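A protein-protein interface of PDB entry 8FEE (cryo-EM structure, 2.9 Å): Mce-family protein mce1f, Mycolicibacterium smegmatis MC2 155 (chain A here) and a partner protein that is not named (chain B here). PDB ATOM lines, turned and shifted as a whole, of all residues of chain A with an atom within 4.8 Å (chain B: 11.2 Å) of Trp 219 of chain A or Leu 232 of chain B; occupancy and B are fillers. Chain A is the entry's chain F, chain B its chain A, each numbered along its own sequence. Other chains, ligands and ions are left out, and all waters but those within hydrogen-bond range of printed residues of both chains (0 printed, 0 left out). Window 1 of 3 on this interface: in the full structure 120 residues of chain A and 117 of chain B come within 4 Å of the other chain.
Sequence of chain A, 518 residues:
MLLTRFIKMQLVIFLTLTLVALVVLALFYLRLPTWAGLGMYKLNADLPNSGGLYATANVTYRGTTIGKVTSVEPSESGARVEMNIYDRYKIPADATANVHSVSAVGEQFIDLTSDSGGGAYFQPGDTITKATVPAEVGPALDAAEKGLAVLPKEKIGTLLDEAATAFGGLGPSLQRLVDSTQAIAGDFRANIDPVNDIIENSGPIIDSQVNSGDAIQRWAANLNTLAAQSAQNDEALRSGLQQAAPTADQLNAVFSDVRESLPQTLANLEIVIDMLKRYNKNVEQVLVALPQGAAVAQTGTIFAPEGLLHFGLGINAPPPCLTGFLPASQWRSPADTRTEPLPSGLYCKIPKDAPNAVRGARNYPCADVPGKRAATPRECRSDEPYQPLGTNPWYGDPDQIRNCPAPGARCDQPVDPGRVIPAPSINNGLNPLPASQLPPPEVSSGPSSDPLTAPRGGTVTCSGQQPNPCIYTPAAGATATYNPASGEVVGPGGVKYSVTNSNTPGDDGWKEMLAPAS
Of chain B, only Leu 232 comes within 4 Å of Trp 219 of chain A. Leu 232 of chain B touches just these residues of chain A: Trp 219 and Leu 223. Ile 216 of chain A touches two residues of chain B. Of chain B, only Ala 228 (3.9 Å) and Asp 231 (3.8 Å) come within 4 Å of Ala 220 of chain A. Ala 221 of chain A touches one residue of chain B. No residue of chain B comes within 4 Å of Asn 222 of chain A. Of the printed residues of chain B, Leu 223 of chain A touches Leu 232. Printed residues of chain A within 4 Å of Asp 227 of chain B: Gln 217. Of the printed residues of chain A, Tyr 225 of chain B touches Ile 216 (3.5 Å). Printed residues of chain B within 4 Å of Gln 217 of chain A: Asp 227 and Ala 228. Asn 238 of chain B touches none of the printed residues of chain A. The nearest printed residue of chain A that does not touch Asp 227 of chain B is Ala 220 of chain A (7.1 Å).
Of the 9 printed residues of chain A, 6 touch a printed residue of chain B. Printed residues of chain A that touch a printed residue of chain B: Ile 216, Gln 217, Trp 219, Ala 220, Ala 221 and Leu 223. Of the 19 printed residues of chain B, 6 touch a printed residue of chain A. Hydrophobic or aromatic side chains of chain B that line the printed part of chain A: Val 224, Tyr 225, Ala 228 and Leu 232.
Among the printed residues, merely in contact across the chains: Ala 221 of chain A with Asp 231 of chain B (3.4 Å), Ile 216 of chain A with Tyr 225 of chain B (3.5 Å), Gln 217 of chain A with Asp 227 of chain B (3.5 Å), Ile 216 of chain A with Val 224 of chain B (3.6 Å), Trp 219 of chain A with Leu 232 of chain B (3.7 Å), Gln 217 of chain A with Ala 228 of chain B (3.7 Å), Ala 220 of chain A with Asp 231 of chain B (3.8 Å), Ala 220 of chain A with Ala 228 of chain B (3.9 Å) and Leu 223 of chain A with Leu 232 of chain B (3.9 Å).
The backbone carbonyl oxygen (O) of Tyr 225 of chain B is in hydrogen-bond range of the side-chain hydroxyl (OG) of Ser 229 of chain B, 3.1 Å away.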
ATOM      1  N   ALA A 215     -20.868 -24.414  29.074  1.00  0.00           N
ATOM      2  CA  ALA A 215     -20.629 -23.102  29.662  1.00  0.00           C
ATOM      3  C   ALA A 215     -19.193 -22.660  29.431  1.00  0.00           C
ATOM      4  O   ALA A 215     -18.943 -21.485  29.130  1.00  0.00           O
ATOM      5  CB  ALA A 215     -20.952 -23.126  31.156  1.00  0.00           C
ATOM      6  N   ILE A 216     -18.232 -23.570  29.596  1.00  0.00           N
ATOM      7  CA  ILE A 216     -16.848 -23.145  29.444  1.00  0.00           C
ATOM      8  C   ILE A 216     -16.541 -22.882  27.977  1.00  0.00           C
ATOM      9  O   ILE A 216     -15.776 -21.966  27.659  1.00  0.00           O
ATOM     10  CB  ILE A 216     -15.869 -24.145  30.089  1.00  0.00           C
ATOM     11  CG1 ILE A 216     -15.775 -25.451  29.308  1.00  0.00           C
ATOM     12  CG2 ILE A 216     -16.256 -24.412  31.535  1.00  0.00           C
ATOM     13  CD1 ILE A 216     -14.807 -26.416  29.924  1.00  0.00           C
ATOM     14  N   GLN A 217     -17.140 -23.648  27.058  1.00  0.00           N
ATOM     15  CA  GLN A 217     -16.990 -23.329  25.640  1.00  0.00           C
ATOM     16  C   GLN A 217     -17.569 -21.955  25.326  1.00  0.00           C
ATOM     17  O   GLN A 217     -16.970 -21.173  24.574  1.00  0.00           O
ATOM     18  CB  GLN A 217     -17.652 -24.402  24.776  1.00  0.00           C
ATOM     19  CG  GLN A 217     -16.976 -25.757  24.842  1.00  0.00           C
ATOM     20  CD  GLN A 217     -17.556 -26.741  23.850  1.00  0.00           C
ATOM     21  OE1 GLN A 217     -18.356 -26.374  22.989  1.00  0.00           O
ATOM     22  NE2 GLN A 217     -17.158 -28.002  23.966  1.00  0.00           N
ATOM     23  N   ARG A 218     -18.724 -21.631  25.921  1.00  0.00           N
ATOM     24  CA  ARG A 218     -19.340 -20.333  25.663  1.00  0.00           C
ATOM     25  C   ARG A 218     -18.481 -19.193  26.197  1.00  0.00           C
ATOM     26  O   ARG A 218     -18.258 -18.198  25.495  1.00  0.00           O
ATOM     27  CB  ARG A 218     -20.740 -20.282  26.273  1.00  0.00           C
ATOM     28  CG  ARG A 218     -21.472 -18.977  26.004  1.00  0.00           C
ATOM     29  CD  ARG A 218     -21.518 -18.671  24.516  1.00  0.00           C
ATOM     30  NE  ARG A 218     -22.188 -17.407  24.237  1.00  0.00           N
ATOM     31  CZ  ARG A 218     -22.395 -16.924  23.020  1.00  0.00           C
ATOM     32  NH1 ARG A 218     -21.991 -17.574  21.941  1.00  0.00           N
ATOM     33  NH2 ARG A 218     -23.020 -15.759  22.882  1.00  0.00           N
ATOM     34  N   TRP A 219     -17.986 -19.309  27.434  1.00  0.00           N
ATOM     35  CA  TRP A 219     -17.179 -18.198  27.931  1.00  0.00           C
ATOM     36  C   TRP A 219     -15.814 -18.150  27.264  1.00  0.00           C
ATOM     37  O   TRP A 219     -15.234 -17.069  27.176  1.00  0.00           O
ATOM     38  CB  TRP A 219     -17.058 -18.195  29.470  1.00  0.00           C
ATOM     39  CG  TRP A 219     -16.256 -19.267  30.190  1.00  0.00           C
ATOM     40  CD1 TRP A 219     -16.759 -20.197  31.051  1.00  0.00           C
ATOM     41  CD2 TRP A 219     -14.828 -19.461  30.191  1.00  0.00           C
ATOM     42  NE1 TRP A 219     -15.751 -20.979  31.554  1.00  0.00           N
ATOM     43  CE2 TRP A 219     -14.557 -20.554  31.040  1.00  0.00           C
ATOM     44  CE3 TRP A 219     -13.757 -18.833  29.547  1.00  0.00           C
ATOM     45  CZ2 TRP A 219     -13.267 -21.029  31.257  1.00  0.00           C
ATOM     46  CZ3 TRP A 219     -12.480 -19.313  29.757  1.00  0.00           C
ATOM     47  CH2 TRP A 219     -12.245 -20.398  30.607  1.00  0.00           C
ATOM     48  N   ALA A 220     -15.301 -19.275  26.759  1.00  0.00           N
ATOM     49  CA  ALA A 220     -14.069 -19.228  25.980  1.00  0.00           C
ATOM     50  C   ALA A 220     -14.273 -18.451  24.687  1.00  0.00           C
ATOM     51  O   ALA A 220     -13.451 -17.599  24.326  1.00  0.00           O
ATOM     52  CB  ALA A 220     -13.575 -20.644  25.689  1.00  0.00           C
ATOM     53  N   ALA A 221     -15.372 -18.727  23.977  1.00  0.00           N
ATOM     54  CA  ALA A 221     -15.658 -17.979  22.753  1.00  0.00           C
ATOM     55  C   ALA A 221     -15.889 -16.500  23.046  1.00  0.00           C
ATOM     56  O   ALA A 221     -15.422 -15.628  22.299  1.00  0.00           O
ATOM     57  CB  ALA A 221     -16.868 -18.582  22.041  1.00  0.00           C
ATOM     58  N   ASN A 222     -16.599 -16.197  24.137  1.00  0.00           N
ATOM     59  CA  ASN A 222     -16.847 -14.803  24.494  1.00  0.00           C
ATOM     60  C   ASN A 222     -15.559 -14.083  24.873  1.00  0.00           C
ATOM     61  O   ASN A 222     -15.366 -12.915  24.512  1.00  0.00           O
ATOM     62  CB  ASN A 222     -17.860 -14.730  25.631  1.00  0.00           C
ATOM     63  CG  ASN A 222     -19.257 -15.094  25.186  1.00  0.00           C
ATOM     64  OD1 ASN A 222     -19.580 -15.031  24.000  1.00  0.00           O
ATOM     65  ND2 ASN A 222     -20.098 -15.481  26.136  1.00  0.00           N
ATOM     66  N   LEU A 223     -14.676 -14.752  25.617  1.00  0.00           N
ATOM     67  CA  LEU A 223     -13.388 -14.161  25.957  1.00  0.00           C
ATOM     68  C   LEU A 223     -12.552 -13.924  24.711  1.00  0.00           C
ATOM     69  O   LEU A 223     -11.869 -12.903  24.602  1.00  0.00           O
ATOM     70  CB  LEU A 223     -12.642 -15.059  26.943  1.00  0.00           C
ATOM     71  CG  LEU A 223     -11.297 -14.538  27.447  1.00  0.00           C
ATOM     72  CD1 LEU A 223     -11.496 -13.302  28.306  1.00  0.00           C
ATOM     73  CD2 LEU A 223     -10.556 -15.618  28.216  1.00  0.00           C
ATOM     74  N   LEU B 221     -13.637 -34.788  29.831  1.00  0.00           N
ATOM     75  CA  LEU B 221     -13.049 -33.477  30.075  1.00  0.00           C
ATOM     76  C   LEU B 221     -11.965 -33.160  29.059  1.00  0.00           C
ATOM     77  O   LEU B 221     -11.824 -32.010  28.635  1.00  0.00           O
ATOM     78  CB  LEU B 221     -12.490 -33.406  31.494  1.00  0.00           C
ATOM     79  CG  LEU B 221     -12.078 -32.006  31.941  1.00  0.00           C
ATOM     80  CD1 LEU B 221     -13.185 -31.018  31.633  1.00  0.00           C
ATOM     81  CD2 LEU B 221     -11.739 -31.989  33.419  1.00  0.00           C
ATOM     82  N   VAL B 224     -13.767 -32.080  25.971  1.00  0.00           N
ATOM     83  CA  VAL B 224     -14.326 -30.742  26.167  1.00  0.00           C
ATOM     84  C   VAL B 224     -13.237 -29.683  26.032  1.00  0.00           C
ATOM     85  O   VAL B 224     -13.410 -28.667  25.345  1.00  0.00           O
ATOM     86  CB  VAL B 224     -15.038 -30.652  27.527  1.00  0.00           C
ATOM     87  CG1 VAL B 224     -15.399 -29.226  27.829  1.00  0.00           C
ATOM     88  CG2 VAL B 224     -16.291 -31.506  27.524  1.00  0.00           C
ATOM     89  N   TYR B 225     -12.090 -29.913  26.676  1.00  0.00           N
ATOM     90  CA  TYR B 225     -11.001 -28.946  26.615  1.00  0.00           C
ATOM     91  C   TYR B 225     -10.403 -28.871  25.218  1.00  0.00           C
ATOM     92  O   TYR B 225     -10.002 -27.795  24.771  1.00  0.00           O
ATOM     93  CB  TYR B 225      -9.922 -29.295  27.638  1.00  0.00           C
ATOM     94  CG  TYR B 225     -10.275 -28.947  29.065  1.00  0.00           C
ATOM     95  CD1 TYR B 225     -11.300 -28.059  29.350  1.00  0.00           C
ATOM     96  CD2 TYR B 225      -9.571 -29.496  30.127  1.00  0.00           C
ATOM     97  CE1 TYR B 225     -11.620 -27.735  30.652  1.00  0.00           C
ATOM     98  CE2 TYR B 225      -9.884 -29.176  31.432  1.00  0.00           C
ATOM     99  CZ  TYR B 225     -10.910 -28.295  31.688  1.00  0.00           C
ATOM    100  OH  TYR B 225     -11.228 -27.973  32.986  1.00  0.00           O
ATOM    101  N   ALA B 226     -10.321 -30.003  24.516  1.00  0.00           N
ATOM    102  CA  ALA B 226      -9.818 -29.976  23.148  1.00  0.00           C
ATOM    103  C   ALA B 226     -10.747 -29.192  22.236  1.00  0.00           C
ATOM    104  O   ALA B 226     -10.286 -28.530  21.299  1.00  0.00           O
ATOM    105  CB  ALA B 226      -9.630 -31.400  22.627  1.00  0.00           C
ATOM    106  N   ASP B 227     -12.057 -29.262  22.484  1.00  0.00           N
ATOM    107  CA  ASP B 227     -12.992 -28.454  21.708  1.00  0.00           C
ATOM    108  C   ASP B 227     -12.875 -26.973  22.054  1.00  0.00           C
ATOM    109  O   ASP B 227     -12.956 -26.115  21.167  1.00  0.00           O
ATOM    110  CB  ASP B 227     -14.420 -28.947  21.933  1.00  0.00           C
ATOM    111  CG  ASP B 227     -14.636 -30.358  21.427  1.00  0.00           C
ATOM    112  OD1 ASP B 227     -13.712 -30.913  20.796  1.00  0.00           O
ATOM    113  OD2 ASP B 227     -15.728 -30.915  21.663  1.00  0.00           O
ATOM    114  N   ALA B 228     -12.688 -26.649  23.333  1.00  0.00           N
ATOM    115  CA  ALA B 228     -12.737 -25.263  23.789  1.00  0.00           C
ATOM    116  C   ALA B 228     -11.379 -24.567  23.784  1.00  0.00           C
ATOM    117  O   ALA B 228     -11.315 -23.370  24.083  1.00  0.00           O
ATOM    118  CB  ALA B 228     -13.332 -25.194  25.198  1.00  0.00           C
ATOM    119  N   SER B 229     -10.297 -25.284  23.470  1.00  0.00           N
ATOM    120  CA  SER B 229      -8.963 -24.689  23.558  1.00  0.00           C
ATOM    121  C   SER B 229      -8.676 -23.603  22.522  1.00  0.00           C
ATOM    122  O   SER B 229      -8.085 -22.579  22.903  1.00  0.00           O
ATOM    123  CB  SER B 229      -7.903 -25.794  23.530  1.00  0.00           C
ATOM    124  OG  SER B 229      -8.141 -26.729  22.495  1.00  0.00           O
ATOM    125  N   PRO B 230      -8.984 -23.764  21.219  1.00  0.00           N
ATOM    126  CA  PRO B 230      -8.561 -22.722  20.257  1.00  0.00           C
ATOM    127  C   PRO B 230      -9.098 -21.333  20.560  1.00  0.00           C
ATOM    128  O   PRO B 230      -8.351 -20.346  20.454  1.00  0.00           O
ATOM    129  CB  PRO B 230      -9.092 -23.251  18.918  1.00  0.00           C
ATOM    130  CG  PRO B 230      -9.207 -24.704  19.107  1.00  0.00           C
ATOM    131  CD  PRO B 230      -9.664 -24.868  20.517  1.00  0.00           C
ATOM    132  N   ASP B 231     -10.373 -21.227  20.941  1.00  0.00           N
ATOM    133  CA  ASP B 231     -10.925 -19.929  21.306  1.00  0.00           C
ATOM    134  C   ASP B 231     -10.222 -19.362  22.530  1.00  0.00           C
ATOM    135  O   ASP B 231      -9.897 -18.168  22.572  1.00  0.00           O
ATOM    136  CB  ASP B 231     -12.428 -20.045  21.556  1.00  0.00           C
ATOM    137  CG  ASP B 231     -13.212 -20.288  20.283  1.00  0.00           C
ATOM    138  OD1 ASP B 231     -12.583 -20.418  19.212  1.00  0.00           O
ATOM    139  OD2 ASP B 231     -14.457 -20.347  20.354  1.00  0.00           O
ATOM    140  N   LEU B 232      -9.962 -20.209  23.530  1.00  0.00           N
ATOM    141  CA  LEU B 232      -9.281 -19.740  24.731  1.00  0.00           C
ATOM    142  C   LEU B 232      -7.883 -19.237  24.405  1.00  0.00           C
ATOM    143  O   LEU B 232      -7.445 -18.222  24.947  1.00  0.00           O
ATOM    144  CB  LEU B 232      -9.210 -20.847  25.779  1.00  0.00           C
ATOM    145  CG  LEU B 232      -8.547 -20.381  27.079  1.00  0.00           C
ATOM    146  CD1 LEU B 232      -9.396 -19.323  27.767  1.00  0.00           C
ATOM    147  CD2 LEU B 232      -8.252 -21.539  28.016  1.00  0.00           C
ATOM    148  N   PHE B 233      -7.178 -19.918  23.504  1.00  0.00           N
ATOM    149  CA  PHE B 233      -5.801 -19.530  23.218  1.00  0.00           C
ATOM    150  C   PHE B 233      -5.731 -18.274  22.356  1.00  0.00           C
ATOM    151  O   PHE B 233      -4.834 -17.444  22.543  1.00  0.00           O
ATOM    152  CB  PHE B 233      -5.050 -20.690  22.567  1.00  0.00           C
ATOM    153  CG  PHE B 233      -4.528 -21.693  23.554  1.00  0.00           C
ATOM    154  CD1 PHE B 233      -3.563 -21.333  24.477  1.00  0.00           C
ATOM    155  CD2 PHE B 233      -5.003 -22.993  23.560  1.00  0.00           C
ATOM    156  CE1 PHE B 233      -3.081 -22.248  25.390  1.00  0.00           C
ATOM    157  CE2 PHE B 233      -4.525 -23.914  24.470  1.00  0.00           C
ATOM    158  CZ  PHE B 233      -3.563 -23.541  25.386  1.00  0.00           C
ATOM    159  N   ASP B 234      -6.667 -18.101  21.417  1.00  0.00           N
ATOM    160  CA  ASP B 234      -6.730 -16.835  20.688  1.00  0.00           C
ATOM    161  C   ASP B 234      -7.066 -15.683  21.631  1.00  0.00           C
ATOM    162  O   ASP B 234      -6.462 -14.597  21.557  1.00  0.00           O
ATOM    163  CB  ASP B 234      -7.755 -16.925  19.559  1.00  0.00           C
ATOM    164  CG  ASP B 234      -7.382 -17.959  18.518  1.00  0.00           C
ATOM    165  OD1 ASP B 234      -6.314 -18.590  18.663  1.00  0.00           O
ATOM    166  OD2 ASP B 234      -8.156 -18.142  17.556  1.00  0.00           O
ATOM    167  N   GLY B 235      -8.029 -15.909  22.531  1.00  0.00           N
ATOM    168  CA  GLY B 235      -8.334 -14.913  23.535  1.00  0.00           C
ATOM    169  C   GLY B 235      -7.156 -14.622  24.436  1.00  0.00           C
ATOM    170  O   GLY B 235      -6.963 -13.486  24.856  1.00  0.00           O
ATOM    171  N   LEU B 236      -6.341 -15.638  24.728  1.00  0.00           N
ATOM    172  CA  LEU B 236      -5.160 -15.425  25.556  1.00  0.00           C
ATOM    173  C   LEU B 236      -4.099 -14.628  24.813  1.00  0.00           C
ATOM    174  O   LEU B 236      -3.410 -13.806  25.417  1.00  0.00           O
ATOM    175  CB  LEU B 236      -4.594 -16.761  26.036  1.00  0.00           C
ATOM    176  CG  LEU B 236      -5.331 -17.439  27.192  1.00  0.00           C
ATOM    177  CD1 LEU B 236      -4.549 -18.640  27.696  1.00  0.00           C
ATOM    178  CD2 LEU B 236      -5.587 -16.450  28.317  1.00  0.00           C
ATOM    179  N   ASP B 237      -3.953 -14.849  23.504  1.00  0.00           N
ATOM    180  CA  ASP B 237      -3.039 -14.026  22.709  1.00  0.00           C
ATOM    181  C   ASP B 237      -3.433 -12.555  22.776  1.00  0.00           C
ATOM    182  O   ASP B 237      -2.615 -11.681  23.106  1.00  0.00           O
ATOM    183  CB  ASP B 237      -3.030 -14.502  21.256  1.00  0.00           C
ATOM    184  CG  ASP B 237      -1.868 -15.418  20.946  1.00  0.00           C
ATOM    185  OD1 ASP B 237      -0.784 -15.222  21.532  1.00  0.00           O
ATOM    186  OD2 ASP B 237      -2.037 -16.332  20.113  1.00  0.00           O
ATOM    187  N   ASN B 238      -4.695 -12.264  22.466  1.00  0.00           N
ATOM    188  CA  ASN B 238      -5.112 -10.865  22.448  1.00  0.00           C
ATOM    189  C   ASN B 238      -5.172 -10.279  23.858  1.00  0.00           C
ATOM    190  O   ASN B 238      -4.920  -9.079  24.048  1.00  0.00           O
ATOM    191  CB  ASN B 238      -6.446 -10.746  21.724  1.00  0.00           C
ATOM    192  CG  ASN B 238      -6.356 -11.195  20.278  1.00  0.00           C
ATOM    193  OD1 ASN B 238      -5.316 -11.049  19.637  1.00  0.00           O
ATOM    194  ND2 ASN B 238      -7.438 -11.767  19.766  1.00  0.00           N
ATOM    195  N   ALA B 239      -5.463 -11.111  24.861  1.00  0.00           N
ATOM    196  CA  ALA B 239      -5.397 -10.672  26.246  1.00  0.00           C
ATOM    197  C   ALA B 239      -3.966 -10.394  26.669  1.00  0.00           C
ATOM    198  O   ALA B 239      -3.734  -9.524  27.506  1.00  0.00           O
ATOM    199  CB  ALA B 239      -6.036 -11.718  27.157  1.00  0.00           C
ATOM    200  N   VAL B 240      -2.997 -11.109  26.099  1.00  0.00           N
ATOM    201  CA  VAL B 240      -1.593 -10.805  26.348  1.00  0.00           C
ATOM    202  C   VAL B 240      -1.241  -9.449  25.763  1.00  0.00           C
ATOM    203  O   VAL B 240      -0.525  -8.656  26.387  1.00  0.00           O
ATOM    204  CB  VAL B 240      -0.696 -11.924  25.786  1.00  0.00           C
ATOM    205  CG1 VAL B 240       0.712 -11.427  25.563  1.00  0.00           C
ATOM    206  CG2 VAL B 240      -0.657 -13.075  26.750  1.00  0.00           C
ATOM    207  N   THR B 241      -1.726  -9.166  24.553  1.00  0.00           N
ATOM    208  CA  THR B 241      -1.491  -7.847  23.963  1.00  0.00           C
ATOM    209  C   THR B 241      -2.059  -6.732  24.846  1.00  0.00           C
ATOM    210  O   THR B 241      -1.350  -5.776  25.202  1.00  0.00           O
ATOM    211  CB  THR B 241      -2.097  -7.784  22.560  1.00  0.00           C
ATOM    212  OG1 THR B 241      -1.287  -8.542  21.654  1.00  0.00           O
ATOM    213  CG2 THR B 241      -2.174  -6.345  22.075  1.00  0.00           C
